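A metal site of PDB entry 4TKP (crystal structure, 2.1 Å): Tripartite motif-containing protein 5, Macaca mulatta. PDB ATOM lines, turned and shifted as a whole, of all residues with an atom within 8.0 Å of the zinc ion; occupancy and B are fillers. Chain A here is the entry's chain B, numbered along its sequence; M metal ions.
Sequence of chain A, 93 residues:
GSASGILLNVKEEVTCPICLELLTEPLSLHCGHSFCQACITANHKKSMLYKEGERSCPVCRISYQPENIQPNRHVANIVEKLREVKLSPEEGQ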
ATOM      1  N   LEU A  29     -27.271  -0.424  -7.956  1.00  0.00           N
ATOM      2  CA  LEU A  29     -27.723   0.503  -8.992  1.00  0.00           C
ATOM      3  C   LEU A  29     -29.214   0.712  -8.842  1.00  0.00           C
ATOM      4  O   LEU A  29     -29.897  -0.116  -8.231  1.00  0.00           O
ATOM      5  CB  LEU A  29     -27.422  -0.067 -10.372  1.00  0.00           C
ATOM      6  CG  LEU A  29     -25.972  -0.447 -10.679  1.00  0.00           C
ATOM      7  CD1 LEU A  29     -25.890  -1.179 -11.993  1.00  0.00           C
ATOM      8  CD2 LEU A  29     -25.106   0.790 -10.731  1.00  0.00           C
ATOM      9  N   HIS A  30     -29.729   1.795  -9.396  1.00  0.00           N
ATOM     10  CA  HIS A  30     -31.152   2.116  -9.295  1.00  0.00           C
ATOM     11  C   HIS A  30     -32.033   1.074  -9.985  1.00  0.00           C
ATOM     12  O   HIS A  30     -33.239   1.018  -9.741  1.00  0.00           O
ATOM     13  CB  HIS A  30     -31.446   3.519  -9.846  1.00  0.00           C
ATOM     14  CG  HIS A  30     -31.061   3.706 -11.275  1.00  0.00           C
ATOM     15  ND1 HIS A  30     -31.849   4.398 -12.179  1.00  0.00           N
ATOM     16  CD2 HIS A  30     -29.963   3.315 -11.975  1.00  0.00           C
ATOM     17  CE1 HIS A  30     -31.259   4.406 -13.355  1.00  0.00           C
ATOM     18  NE2 HIS A  30     -30.115   3.753 -13.257  1.00  0.00           N
ATOM     19  N   CYS A  31     -31.438   0.259 -10.838  1.00  0.00           N
ATOM     20  CA  CYS A  31     -32.160  -0.814 -11.505  1.00  0.00           C
ATOM     21  C   CYS A  31     -32.362  -2.011 -10.574  1.00  0.00           C
ATOM     22  O   CYS A  31     -33.142  -2.916 -10.876  1.00  0.00           O
ATOM     23  CB  CYS A  31     -31.421  -1.257 -12.770  1.00  0.00           C
ATOM     24  SG  CYS A  31     -29.702  -1.699 -12.481  1.00  0.00           S
ATOM     25  N   GLY A  32     -31.656  -2.008  -9.451  1.00  0.00           N
ATOM     26  CA  GLY A  32     -31.807  -3.063  -8.461  1.00  0.00           C
ATOM     27  C   GLY A  32     -30.670  -4.069  -8.430  1.00  0.00           C
ATOM     28  O   GLY A  32     -30.606  -4.916  -7.535  1.00  0.00           O
ATOM     29  N   HIS A  33     -29.771  -3.965  -9.395  1.00  0.00           N
ATOM     30  CA  HIS A  33     -28.632  -4.875  -9.467  1.00  0.00           C
ATOM     31  C   HIS A  33     -27.458  -4.353  -8.639  1.00  0.00           C
ATOM     32  O   HIS A  33     -27.194  -3.157  -8.595  1.00  0.00           O
ATOM     33  CB  HIS A  33     -28.210  -5.099 -10.925  1.00  0.00           C
ATOM     34  CG  HIS A  33     -29.243  -5.804 -11.737  1.00  0.00           C
ATOM     35  ND1 HIS A  33     -29.715  -5.298 -12.930  1.00  0.00           N
ATOM     36  CD2 HIS A  33     -29.899  -6.966 -11.542  1.00  0.00           C
ATOM     37  CE1 HIS A  33     -30.619  -6.118 -13.436  1.00  0.00           C
ATOM     38  NE2 HIS A  33     -30.750  -7.142 -12.606  1.00  0.00           N
ATOM     39  N   SER A  34     -26.746  -5.274  -7.987  1.00  0.00           N
ATOM     40  CA  SER A  34     -25.658  -4.910  -7.099  1.00  0.00           C
ATOM     41  C   SER A  34     -24.378  -5.684  -7.414  1.00  0.00           C
ATOM     42  O   SER A  34     -24.419  -6.773  -7.974  1.00  0.00           O
ATOM     43  CB  SER A  34     -26.055  -5.141  -5.641  1.00  0.00           C
ATOM     44  OG  SER A  34     -27.301  -4.529  -5.356  1.00  0.00           O
ATOM     45  N   PHE A  35     -23.244  -5.102  -7.039  1.00  0.00           N
ATOM     46  CA  PHE A  35     -21.937  -5.690  -7.312  1.00  0.00           C
ATOM     47  C   PHE A  35     -21.013  -5.457  -6.135  1.00  0.00           C
ATOM     48  O   PHE A  35     -21.240  -4.555  -5.333  1.00  0.00           O
ATOM     49  CB  PHE A  35     -21.320  -5.056  -8.576  1.00  0.00           C
ATOM     50  CG  PHE A  35     -22.258  -5.018  -9.754  1.00  0.00           C
ATOM     51  CD1 PHE A  35     -23.160  -3.981  -9.916  1.00  0.00           C
ATOM     52  CD2 PHE A  35     -22.213  -6.015 -10.711  1.00  0.00           C
ATOM     53  CE1 PHE A  35     -24.014  -3.948 -10.993  1.00  0.00           C
ATOM     54  CE2 PHE A  35     -23.065  -5.978 -11.801  1.00  0.00           C
ATOM     55  CZ  PHE A  35     -23.957  -4.945 -11.942  1.00  0.00           C
ATOM     56  N   SER A  56     -23.097   2.194 -17.732  1.00  0.00           N
ATOM     57  CA  SER A  56     -24.159   1.221 -18.016  1.00  0.00           C
ATOM     58  C   SER A  56     -24.057  -0.018 -17.131  1.00  0.00           C
ATOM     59  O   SER A  56     -22.963  -0.534 -16.894  1.00  0.00           O
ATOM     60  CB  SER A  56     -24.121   0.810 -19.495  1.00  0.00           C
ATOM     61  OG  SER A  56     -25.135  -0.149 -19.786  1.00  0.00           O
ATOM     62  N   CYS A  57     -25.193  -0.489 -16.624  1.00  0.00           N
ATOM     63  CA  CYS A  57     -25.237  -1.703 -15.815  1.00  0.00           C
ATOM     64  C   CYS A  57     -24.731  -2.897 -16.620  1.00  0.00           C
ATOM     65  O   CYS A  57     -25.225  -3.159 -17.705  1.00  0.00           O
ATOM     66  CB  CYS A  57     -26.652  -1.988 -15.325  1.00  0.00           C
ATOM     67  SG  CYS A  57     -26.816  -3.529 -14.379  1.00  0.00           S
ATOM     68  N   PRO A  58     -23.741  -3.622 -16.079  1.00  0.00           N
ATOM     69  CA  PRO A  58     -23.209  -4.812 -16.740  1.00  0.00           C
ATOM     70  C   PRO A  58     -24.289  -5.870 -16.986  1.00  0.00           C
ATOM     71  O   PRO A  58     -24.158  -6.680 -17.898  1.00  0.00           O
ATOM     72  CB  PRO A  58     -22.170  -5.335 -15.740  1.00  0.00           C
ATOM     73  CG  PRO A  58     -21.748  -4.126 -14.987  1.00  0.00           C
ATOM     74  CD  PRO A  58     -22.983  -3.273 -14.867  1.00  0.00           C
ATOM     75  N   VAL A  59     -25.342  -5.839 -16.172  1.00  0.00           N
ATOM     76  CA  VAL A  59     -26.413  -6.838 -16.264  1.00  0.00           C
ATOM     77  C   VAL A  59     -27.566  -6.423 -17.188  1.00  0.00           C
ATOM     78  O   VAL A  59     -27.874  -7.128 -18.146  1.00  0.00           O
ATOM     79  CB  VAL A  59     -26.969  -7.192 -14.873  1.00  0.00           C
ATOM     80  CG1 VAL A  59     -28.160  -8.138 -14.992  1.00  0.00           C
ATOM     81  CG2 VAL A  59     -25.886  -7.806 -14.004  1.00  0.00           C
ATOM     82  N   CYS A  60     -28.200  -5.292 -16.890  1.00  0.00           N
ATOM     83  CA  CYS A  60     -29.394  -4.885 -17.626  1.00  0.00           C
ATOM     84  C   CYS A  60     -29.147  -3.759 -18.630  1.00  0.00           C
ATOM     85  O   CYS A  60     -30.028  -3.425 -19.421  1.00  0.00           O
ATOM     86  CB  CYS A  60     -30.508  -4.473 -16.651  1.00  0.00           C
ATOM     87  SG  CYS A  60     -30.236  -2.880 -15.854  1.00  0.00           S
ATOM     88  N   ARG A  61     -27.957  -3.165 -18.561  1.00  0.00           N
ATOM     89  CA  ARG A  61     -27.530  -2.122 -19.499  1.00  0.00           C
ATOM     90  C   ARG A  61     -28.287  -0.792 -19.374  1.00  0.00           C
ATOM     91  O   ARG A  61     -28.090   0.108 -20.196  1.00  0.00           O
ATOM     92  CB  ARG A  61     -27.557  -2.627 -20.947  1.00  0.00           C
ATOM     93  CG  ARG A  61     -26.819  -3.939 -21.142  1.00  0.00           C
ATOM     94  CD  ARG A  61     -25.566  -3.766 -21.971  1.00  0.00           C
ATOM     95  NE  ARG A  61     -24.911  -5.050 -22.222  1.00  0.00           N
ATOM     96  CZ  ARG A  61     -25.337  -5.939 -23.122  1.00  0.00           C
ATOM     97  NH1 ARG A  61     -26.416  -5.689 -23.843  1.00  0.00           N
ATOM     98  NH2 ARG A  61     -24.678  -7.079 -23.273  1.00  0.00           N
ATOM     99  N   ILE A  62     -29.130  -0.668 -18.358  1.00  0.00           N
ATOM    100  CA  ILE A  62     -29.757   0.614 -18.062  1.00  0.00           C
ATOM    101  C   ILE A  62     -28.711   1.560 -17.489  1.00  0.00           C
ATOM    102  O   ILE A  62     -28.020   1.226 -16.531  1.00  0.00           O
ATOM    103  CB  ILE A  62     -30.922   0.478 -17.065  1.00  0.00           C
ATOM    104  CG1 ILE A  62     -32.048  -0.364 -17.675  1.00  0.00           C
ATOM    105  CG2 ILE A  62     -31.444   1.842 -16.651  1.00  0.00           C
ATOM    106  CD1 ILE A  62     -33.222  -0.583 -16.736  1.00  0.00           C
ATOM    107  N   SER A  63     -28.585   2.730 -18.099  1.00  0.00           N
ATOM    108  CA  SER A  63     -27.545   3.679 -17.697  1.00  0.00           C
ATOM    109  C   SER A  63     -27.770   4.257 -16.302  1.00  0.00           C
ATOM    110  O   SER A  63     -28.886   4.279 -15.786  1.00  0.00           O
ATOM    111  CB  SER A  63     -27.431   4.811 -18.724  1.00  0.00           C
ATOM    112  OG  SER A  63     -28.640   5.552 -18.818  1.00  0.00           O
ATOM    113  N   TYR A  64     -26.682   4.703 -15.692  1.00  0.00           N
ATOM    114  CA  TYR A  64     -26.715   5.314 -14.369  1.00  0.00           C
ATOM    115  C   TYR A  64     -25.663   6.398 -14.266  1.00  0.00           C
ATOM    116  O   TYR A  64     -24.580   6.287 -14.843  1.00  0.00           O
ATOM    117  CB  TYR A  64     -26.484   4.260 -13.279  1.00  0.00           C
ATOM    118  CG  TYR A  64     -25.093   3.647 -13.294  1.00  0.00           C
ATOM    119  CD1 TYR A  64     -24.812   2.525 -14.068  1.00  0.00           C
ATOM    120  CD2 TYR A  64     -24.067   4.191 -12.528  1.00  0.00           C
ATOM    121  CE1 TYR A  64     -23.548   1.974 -14.078  1.00  0.00           C
ATOM    122  CE2 TYR A  64     -22.803   3.640 -12.538  1.00  0.00           C
ATOM    123  CZ  TYR A  64     -22.542   2.536 -13.308  1.00  0.00           C
ATOM    124  OH  TYR A  64     -21.278   1.985 -13.318  1.00  0.00           O
HETATM  125 ZN    ZN M   1     -29.115  -3.485 -13.905  1.00  0.00          ZN
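Four residues have an atom within 4 Å of the zinc ion: Cys 31, His 33, Cys 57 and Cys 60. The nearest printed residue that does not touch the zinc ion is Val 59 (4.4 Å).
SG of Cys 60 lies close to N of Ile 62 (3.5 Å). O of Ile 62 sits at hydrogen-bond distance from N of Cys 57 (3.3 Å). SG of Cys 57 sits close to N of Val 59 (3.3 Å).
ND1 of His 33 is bound to the zinc ion, at 2.1 Å. The side-chain sulfur (SG) of Cys 60 binds the zinc ion. The zinc ion is bound by SG of Cys 57 (2.3 Å). The zinc ion is bound by SG of Cys 31, 2.4 Å away.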
